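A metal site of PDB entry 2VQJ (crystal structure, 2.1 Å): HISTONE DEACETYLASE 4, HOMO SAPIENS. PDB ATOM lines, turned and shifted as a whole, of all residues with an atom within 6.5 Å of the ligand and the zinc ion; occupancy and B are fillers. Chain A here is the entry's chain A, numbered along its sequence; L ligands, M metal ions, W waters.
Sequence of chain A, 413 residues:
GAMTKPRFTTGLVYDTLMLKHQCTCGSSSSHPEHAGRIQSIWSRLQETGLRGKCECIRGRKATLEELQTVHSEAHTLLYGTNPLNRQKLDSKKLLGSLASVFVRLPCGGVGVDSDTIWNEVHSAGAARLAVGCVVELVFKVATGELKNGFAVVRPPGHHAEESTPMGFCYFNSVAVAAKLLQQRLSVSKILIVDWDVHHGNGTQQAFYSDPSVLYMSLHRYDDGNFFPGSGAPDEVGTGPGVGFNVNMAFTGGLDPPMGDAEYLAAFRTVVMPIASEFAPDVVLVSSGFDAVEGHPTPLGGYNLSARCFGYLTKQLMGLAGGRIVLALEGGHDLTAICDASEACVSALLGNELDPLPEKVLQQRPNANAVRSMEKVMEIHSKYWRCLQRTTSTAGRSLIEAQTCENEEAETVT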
ATOM      1  N   ARG A  37       3.857  33.836 -10.691  1.00  0.00           N
ATOM      2  CA  ARG A  37       4.073  34.842  -9.663  1.00  0.00           C
ATOM      3  C   ARG A  37       4.517  36.201 -10.218  1.00  0.00           C
ATOM      4  O   ARG A  37       3.840  37.213 -10.008  1.00  0.00           O
ATOM      5  CB  ARG A  37       5.099  34.333  -8.647  1.00  0.00           C
ATOM      6  CG  ARG A  37       4.626  33.106  -7.881  1.00  0.00           C
ATOM      7  CD  ARG A  37       5.771  32.311  -7.315  1.00  0.00           C
ATOM      8  NE  ARG A  37       6.522  33.100  -6.357  1.00  0.00           N
ATOM      9  CZ  ARG A  37       7.797  33.476  -6.483  1.00  0.00           C
ATOM     10  NH1 ARG A  37       8.531  33.156  -7.531  1.00  0.00           N
ATOM     11  NH2 ARG A  37       8.338  34.193  -5.514  1.00  0.00           N
ATOM     12  N   PRO A 156      13.799  32.431  -6.867  1.00  0.00           N
ATOM     13  CA  PRO A 156      14.506  33.004  -5.701  1.00  0.00           C
ATOM     14  C   PRO A 156      15.963  32.619  -5.720  1.00  0.00           C
ATOM     15  O   PRO A 156      16.341  31.748  -6.510  1.00  0.00           O
ATOM     16  CB  PRO A 156      13.818  32.352  -4.493  1.00  0.00           C
ATOM     17  CG  PRO A 156      12.623  31.670  -4.988  1.00  0.00           C
ATOM     18  CD  PRO A 156      12.687  31.544  -6.471  1.00  0.00           C
ATOM     19  N   GLY A 157      16.784  33.226  -4.870  1.00  0.00           N
ATOM     20  CA  GLY A 157      18.204  32.886  -4.811  1.00  0.00           C
ATOM     21  C   GLY A 157      18.838  32.622  -3.446  1.00  0.00           C
ATOM     22  O   GLY A 157      19.926  32.089  -3.380  1.00  0.00           O
ATOM     23  N   HIS A 158      18.164  32.975  -2.358  1.00  0.00           N
ATOM     24  CA  HIS A 158      18.827  33.106  -1.046  1.00  0.00           C
ATOM     25  C   HIS A 158      19.204  31.805  -0.324  1.00  0.00           C
ATOM     26  O   HIS A 158      20.014  31.833   0.625  1.00  0.00           O
ATOM     27  CB  HIS A 158      18.048  34.072  -0.120  1.00  0.00           C
ATOM     28  CG  HIS A 158      16.749  33.538   0.394  1.00  0.00           C
ATOM     29  ND1 HIS A 158      16.243  33.909   1.624  1.00  0.00           N
ATOM     30  CD2 HIS A 158      15.846  32.675  -0.131  1.00  0.00           C
ATOM     31  CE1 HIS A 158      15.092  33.307   1.822  1.00  0.00           C
ATOM     32  NE2 HIS A 158      14.827  32.544   0.775  1.00  0.00           N
ATOM     33  N   HIS A 159      18.668  30.673  -0.771  1.00  0.00           N
ATOM     34  CA  HIS A 159      19.043  29.364  -0.246  1.00  0.00           C
ATOM     35  C   HIS A 159      20.211  28.751  -1.019  1.00  0.00           C
ATOM     36  O   HIS A 159      20.819  27.789  -0.529  1.00  0.00           O
ATOM     37  CB  HIS A 159      17.892  28.350  -0.322  1.00  0.00           C
ATOM     38  CG  HIS A 159      16.646  28.748   0.406  1.00  0.00           C
ATOM     39  ND1 HIS A 159      16.630  29.041   1.752  1.00  0.00           N
ATOM     40  CD2 HIS A 159      15.363  28.830  -0.014  1.00  0.00           C
ATOM     41  CE1 HIS A 159      15.393  29.324   2.123  1.00  0.00           C
ATOM     42  NE2 HIS A 159      14.603  29.195   1.067  1.00  0.00           N
ATOM     43  N   MET A 166      19.312  24.650  -3.911  1.00  0.00           N
ATOM     44  CA  MET A 166      18.308  24.121  -2.988  1.00  0.00           C
ATOM     45  C   MET A 166      17.187  25.118  -2.783  1.00  0.00           C
ATOM     46  O   MET A 166      17.345  26.304  -3.061  1.00  0.00           O
ATOM     47  CB  MET A 166      18.908  23.767  -1.618  1.00  0.00           C
ATOM     48  CG  MET A 166      19.832  24.820  -1.059  1.00  0.00           C
ATOM     49  SD  MET A 166      20.477  24.366   0.559  1.00  0.00           S
ATOM     50  CE  MET A 166      19.027  24.730   1.553  1.00  0.00           C
ATOM     51  N   GLY A 167      16.046  24.623  -2.313  1.00  0.00           N
ATOM     52  CA  GLY A 167      14.870  25.454  -2.071  1.00  0.00           C
ATOM     53  C   GLY A 167      14.481  26.277  -3.288  1.00  0.00           C
ATOM     54  O   GLY A 167      14.123  27.440  -3.149  1.00  0.00           O
ATOM     55  N   PHE A 168      14.571  25.683  -4.478  1.00  0.00           N
ATOM     56  CA  PHE A 168      14.201  26.335  -5.743  1.00  0.00           C
ATOM     57  C   PHE A 168      15.214  27.398  -6.197  1.00  0.00           C
ATOM     58  O   PHE A 168      14.946  28.166  -7.112  1.00  0.00           O
ATOM     59  CB  PHE A 168      12.786  26.931  -5.683  1.00  0.00           C
ATOM     60  CG  PHE A 168      11.738  25.978  -5.181  1.00  0.00           C
ATOM     61  CD1 PHE A 168      11.161  26.141  -3.943  1.00  0.00           C
ATOM     62  CD2 PHE A 168      11.333  24.913  -5.977  1.00  0.00           C
ATOM     63  CE1 PHE A 168      10.190  25.246  -3.482  1.00  0.00           C
ATOM     64  CE2 PHE A 168      10.379  24.017  -5.520  1.00  0.00           C
ATOM     65  CZ  PHE A 168       9.805  24.187  -4.270  1.00  0.00           C
ATOM     66  N   CYS A 169      16.380  27.416  -5.557  1.00  0.00           N
ATOM     67  CA  CYS A 169      17.405  28.408  -5.829  1.00  0.00           C
ATOM     68  C   CYS A 169      18.603  27.765  -6.500  1.00  0.00           C
ATOM     69  O   CYS A 169      19.162  26.785  -5.985  1.00  0.00           O
ATOM     70  CB  CYS A 169      17.876  29.068  -4.535  1.00  0.00           C
ATOM     71  SG  CYS A 169      16.535  29.842  -3.612  1.00  0.00           S
ATOM     72  N   ASP A 196      12.090  37.262   3.768  1.00  0.00           N
ATOM     73  CA  ASP A 196      11.458  36.009   3.394  1.00  0.00           C
ATOM     74  C   ASP A 196      11.267  35.221   4.691  1.00  0.00           C
ATOM     75  O   ASP A 196      12.129  35.281   5.581  1.00  0.00           O
ATOM     76  CB  ASP A 196      12.370  35.274   2.420  1.00  0.00           C
ATOM     77  CG  ASP A 196      11.734  34.034   1.837  1.00  0.00           C
ATOM     78  OD1 ASP A 196      11.215  34.108   0.693  1.00  0.00           O
ATOM     79  OD2 ASP A 196      11.757  32.989   2.512  1.00  0.00           O
ATOM     80  N   VAL A 197      10.166  34.481   4.837  1.00  0.00           N
ATOM     81  CA  VAL A 197       9.932  33.752   6.094  1.00  0.00           C
ATOM     82  C   VAL A 197      10.983  32.649   6.412  1.00  0.00           C
ATOM     83  O   VAL A 197      11.129  32.258   7.554  1.00  0.00           O
ATOM     84  CB  VAL A 197       8.463  33.204   6.175  1.00  0.00           C
ATOM     85  CG1 VAL A 197       8.273  31.864   5.402  1.00  0.00           C
ATOM     86  CG2 VAL A 197       8.042  33.068   7.628  1.00  0.00           C
ATOM     87  N   HIS A 198      11.713  32.188   5.405  1.00  0.00           N
ATOM     88  CA  HIS A 198      12.724  31.143   5.574  1.00  0.00           C
ATOM     89  C   HIS A 198      14.106  31.747   5.629  1.00  0.00           C
ATOM     90  O   HIS A 198      14.392  32.746   4.959  1.00  0.00           O
ATOM     91  CB  HIS A 198      12.684  30.139   4.417  1.00  0.00           C
ATOM     92  CG  HIS A 198      11.323  29.554   4.183  1.00  0.00           C
ATOM     93  ND1 HIS A 198      10.432  30.091   3.289  1.00  0.00           N
ATOM     94  CD2 HIS A 198      10.707  28.490   4.743  1.00  0.00           C
ATOM     95  CE1 HIS A 198       9.311  29.394   3.323  1.00  0.00           C
ATOM     96  NE2 HIS A 198       9.456  28.406   4.183  1.00  0.00           N
ATOM     97  N   HIS A 199      14.973  31.176   6.457  1.00  0.00           N
ATOM     98  CA  HIS A 199      16.336  31.675   6.605  1.00  0.00           C
ATOM     99  C   HIS A 199      17.080  31.686   5.276  1.00  0.00           C
ATOM    100  O   HIS A 199      16.996  30.715   4.526  1.00  0.00           O
ATOM    101  CB  HIS A 199      17.095  30.814   7.618  1.00  0.00           C
ATOM    102  CG  HIS A 199      18.502  31.247   7.834  1.00  0.00           C
ATOM    103  ND1 HIS A 199      19.574  30.402   7.681  1.00  0.00           N
ATOM    104  CD2 HIS A 199      19.022  32.444   8.181  1.00  0.00           C
ATOM    105  CE1 HIS A 199      20.690  31.059   7.944  1.00  0.00           C
ATOM    106  NE2 HIS A 199      20.382  32.298   8.260  1.00  0.00           N
ATOM    107  N   PHE A 226      12.078  24.232  11.041  1.00  0.00           N
ATOM    108  CA  PHE A 226      11.415  24.831   9.883  1.00  0.00           C
ATOM    109  C   PHE A 226      12.457  25.016   8.770  1.00  0.00           C
ATOM    110  O   PHE A 226      13.598  25.353   9.044  1.00  0.00           O
ATOM    111  CB  PHE A 226      10.778  26.169  10.313  1.00  0.00           C
ATOM    112  CG  PHE A 226       9.803  26.745   9.319  1.00  0.00           C
ATOM    113  CD1 PHE A 226       8.574  26.131   9.115  1.00  0.00           C
ATOM    114  CD2 PHE A 226      10.094  27.899   8.607  1.00  0.00           C
ATOM    115  CE1 PHE A 226       7.674  26.640   8.198  1.00  0.00           C
ATOM    116  CE2 PHE A 226       9.203  28.422   7.696  1.00  0.00           C
ATOM    117  CZ  PHE A 226       7.989  27.793   7.488  1.00  0.00           C
ATOM    118  N   PHE A 227      12.064  24.763   7.520  1.00  0.00           N
ATOM    119  CA  PHE A 227      13.002  24.855   6.398  1.00  0.00           C
ATOM    120  C   PHE A 227      13.683  26.230   6.323  1.00  0.00           C
ATOM    121  O   PHE A 227      13.017  27.256   6.505  1.00  0.00           O
ATOM    122  CB  PHE A 227      12.263  24.594   5.076  1.00  0.00           C
ATOM    123  CG  PHE A 227      13.161  24.624   3.859  1.00  0.00           C
ATOM    124  CD1 PHE A 227      13.777  23.457   3.419  1.00  0.00           C
ATOM    125  CD2 PHE A 227      13.366  25.804   3.156  1.00  0.00           C
ATOM    126  CE1 PHE A 227      14.598  23.465   2.305  1.00  0.00           C
ATOM    127  CE2 PHE A 227      14.185  25.818   2.031  1.00  0.00           C
ATOM    128  CZ  PHE A 227      14.811  24.645   1.609  1.00  0.00           C
ATOM    129  N   PRO A 228      15.003  26.262   6.014  1.00  0.00           N
ATOM    130  CA  PRO A 228      15.933  25.148   5.764  1.00  0.00           C
ATOM    131  C   PRO A 228      16.561  24.495   6.989  1.00  0.00           C
ATOM    132  O   PRO A 228      17.344  23.561   6.845  1.00  0.00           O
ATOM    133  CB  PRO A 228      17.020  25.800   4.905  1.00  0.00           C
ATOM    134  CG  PRO A 228      17.075  27.188   5.392  1.00  0.00           C
ATOM    135  CD  PRO A 228      15.664  27.559   5.786  1.00  0.00           C
ATOM    136  N   GLY A 288      11.186  38.257   0.131  1.00  0.00           N
ATOM    137  CA  GLY A 288      10.164  37.234  -0.003  1.00  0.00           C
ATOM    138  C   GLY A 288       8.915  37.690   0.701  1.00  0.00           C
ATOM    139  O   GLY A 288       8.970  38.479   1.642  1.00  0.00           O
ATOM    140  N   ASP A 290       6.369  35.342   1.754  1.00  0.00           N
ATOM    141  CA  ASP A 290       5.718  34.174   2.317  1.00  0.00           C
ATOM    142  C   ASP A 290       5.307  34.314   3.792  1.00  0.00           C
ATOM    143  O   ASP A 290       4.588  33.461   4.316  1.00  0.00           O
ATOM    144  CB  ASP A 290       6.503  32.864   2.039  1.00  0.00           C
ATOM    145  CG  ASP A 290       7.991  32.988   2.278  1.00  0.00           C
ATOM    146  OD1 ASP A 290       8.433  34.048   2.770  1.00  0.00           O
ATOM    147  OD2 ASP A 290       8.734  32.006   1.964  1.00  0.00           O
ATOM    148  N   PRO A 298       2.876  24.824   6.760  1.00  0.00           N
ATOM    149  CA  PRO A 298       4.154  24.305   6.280  1.00  0.00           C
ATOM    150  C   PRO A 298       4.968  25.306   5.456  1.00  0.00           C
ATOM    151  O   PRO A 298       6.171  25.461   5.691  1.00  0.00           O
ATOM    152  CB  PRO A 298       3.740  23.092   5.439  1.00  0.00           C
ATOM    153  CG  PRO A 298       2.362  23.364   5.020  1.00  0.00           C
ATOM    154  CD  PRO A 298       1.723  24.181   6.112  1.00  0.00           C
ATOM    155  N   LEU A 299       4.316  25.991   4.507  1.00  0.00           N
ATOM    156  CA  LEU A 299       4.995  26.965   3.653  1.00  0.00           C
ATOM    157  C   LEU A 299       5.358  28.244   4.419  1.00  0.00           C
ATOM    158  O   LEU A 299       6.448  28.772   4.257  1.00  0.00           O
ATOM    159  CB  LEU A 299       4.127  27.350   2.444  1.00  0.00           C
ATOM    160  CG  LEU A 299       4.687  28.408   1.474  1.00  0.00           C
ATOM    161  CD1 LEU A 299       6.077  28.030   0.979  1.00  0.00           C
ATOM    162  CD2 LEU A 299       3.742  28.642   0.283  1.00  0.00           C
ATOM    163  N   GLU A 329      11.978  37.110  -3.500  1.00  0.00           N
ATOM    164  CA  GLU A 329      12.444  35.773  -3.145  1.00  0.00           C
ATOM    165  C   GLU A 329      11.202  34.885  -3.167  1.00  0.00           C
ATOM    166  O   GLU A 329      10.602  34.744  -4.229  1.00  0.00           O
ATOM    167  CB  GLU A 329      13.121  35.791  -1.779  1.00  0.00           C
ATOM    168  CG  GLU A 329      14.338  36.674  -1.713  1.00  0.00           C
ATOM    169  CD  GLU A 329      15.575  36.078  -2.382  1.00  0.00           C
ATOM    170  OE1 GLU A 329      15.494  34.960  -2.944  1.00  0.00           O
ATOM    171  OE2 GLU A 329      16.634  36.730  -2.345  1.00  0.00           O
ATOM    172  N   GLY A 330      10.792  34.336  -2.016  1.00  0.00           N
ATOM    173  CA  GLY A 330       9.598  33.516  -1.889  1.00  0.00           C
ATOM    174  C   GLY A 330       8.292  34.262  -1.762  1.00  0.00           C
ATOM    175  O   GLY A 330       8.201  35.477  -1.993  1.00  0.00           O
ATOM    176  N   GLY A 331       7.250  33.527  -1.408  1.00  0.00           N
ATOM    177  CA  GLY A 331       5.887  34.012  -1.492  1.00  0.00           C
ATOM    178  C   GLY A 331       5.214  33.288  -2.646  1.00  0.00           C
ATOM    179  O   GLY A 331       5.822  33.124  -3.690  1.00  0.00           O
HETATM  180  C1  LIG L   1       6.784  18.511   0.188  1.00  0.00           C
HETATM  181  C2  LIG L   1       5.801  17.810   0.860  1.00  0.00           C
HETATM  182  C3  LIG L   1       5.026  18.443   1.837  1.00  0.00           C
HETATM  183  C4  LIG L   1       5.242  19.778   2.149  1.00  0.00           C
HETATM  184  C5  LIG L   1       6.234  20.479   1.466  1.00  0.00           C
HETATM  185  C6  LIG L   1       7.002  19.860   0.482  1.00  0.00           C
HETATM  186  C7  LIG L   1       8.023  20.545  -0.175  1.00  0.00           C
HETATM  187  C8  LIG L   1       8.540  20.421  -1.402  1.00  0.00           C
HETATM  188  N1  LIG L   1       9.542  21.295  -1.547  1.00  0.00           N
HETATM  189  C9  LIG L   1       9.716  21.971  -0.414  1.00  0.00           C
HETATM  190  C10 LIG L   1      10.740  23.066  -0.078  1.00  0.00           C
HETATM  191  N2  LIG L   1       8.754  21.504   0.495  1.00  0.00           N
HETATM  192  C11 LIG L   1       8.602  22.018   1.861  1.00  0.00           C
HETATM  193  C12 LIG L   1       9.863  22.723   2.264  1.00  0.00           C
HETATM  194  N3  LIG L   1      10.320  23.638   1.205  1.00  0.00           N
HETATM  195  C13 LIG L   1      10.264  24.933   1.491  1.00  0.00           C
HETATM  196  O1  LIG L   1       9.882  25.183   2.631  1.00  0.00           O
HETATM  197  C14 LIG L   1      10.755  26.116   0.670  1.00  0.00           C
HETATM  198  S1  LIG L   1      10.217  27.674   0.968  1.00  0.00           S
HETATM  199  C15 LIG L   1      11.749  26.171  -0.225  1.00  0.00           C
HETATM  200  C16 LIG L   1      12.014  27.427  -0.686  1.00  0.00           C
HETATM  201  C17 LIG L   1      11.251  28.412  -0.147  1.00  0.00           C
HETATM  202  C18 LIG L   1      11.279  29.946  -0.388  1.00  0.00           C
HETATM  203  C19 LIG L   1      11.904  30.367  -1.722  1.00  0.00           C
HETATM  204  F1  LIG L   1      13.101  29.812  -1.879  1.00  0.00           F
HETATM  205  F2  LIG L   1      11.093  30.063  -2.703  1.00  0.00           F
HETATM  206  F3  LIG L   1      12.047  31.676  -1.713  1.00  0.00           F
HETATM  207  O2  LIG L   1       9.964  30.508  -0.278  1.00  0.00           O
HETATM  208  O3  LIG L   1      12.070  30.578   0.668  1.00  0.00           O
HETATM  209 ZN    ZN M   1      10.594  31.475   1.804  1.00  0.00          ZN
HETATM  210  O   HOH W   1       7.702  30.837  -1.109  1.00  0.00           O
HETATM  211  O   HOH W   2      11.877  20.941  -2.651  1.00  0.00           O
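The zinc ion is bound by the side-chain carboxylate of Asp 290 (1.9 Å), the side-chain carboxylate of Asp 196 (2.0 Å), a ring nitrogen (ND1) of His 198 (2.0 Å), an oxygen (O3) of the ligand (2.1 Å) and an oxygen (O2) of the ligand (2.4 Å).
The zinc ion has five donor atoms within binding distance.
N of His 158 is in hydrogen-bond range of OE1 of Glu 329 (3.4 Å).
The side-chain sulfur (SG) of Cys 169 sits close to the backbone NH (N) of Gly 157, 3.6 Å away.
O of Glu 329 sits at hydrogen-bond distance from NH2 of Arg 37 (2.7 Å).
SG of Cys 169 sits close to O of Met 166, 3.7 Å away.
The backbone carbonyl oxygen (O) of Gly 167 is in hydrogen-bond range of the side-chain sulfur (SG) of Cys 169.
ND1 of His 159 sits close to O of His 199, at 3.3 Å.
SG of Cys 169 is in hydrogen-bond range of N of His 158.
NE2 of His 198 sits at hydrogen-bond distance from O of Leu 299, 3.0 Å away.
O3 of the ligand sits close to NE2 of His 158, at 3.4 Å.
A ring nitrogen (NE2) of His 159 lies close to an oxygen (O3) of the ligand, at 2.9 Å.
The backbone carbonyl oxygen (O) of Gly 167 lies close to a fluorine (F1) of the ligand, 2.9 Å away.
A fluorine (F3) of the ligand sits close to the backbone NH (N) of Gly 330.
Residues that only touch the ligand: Pro 156, Phe 168, Cys 169, Phe 227 and Glu 329.
Hydrophobic or aromatic side chains that line the ligand: Pro 156, His 159, Phe 168, His 198 and Phe 227.
The nearest printed residue that does not touch the ligand is Leu 299 (4.2 Å).
Within 4 Å of the zinc ion: Asp 196, His 198 and Asp 290.
The nearest printed residue that does not touch the zinc ion is Val 197 (4.3 Å).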
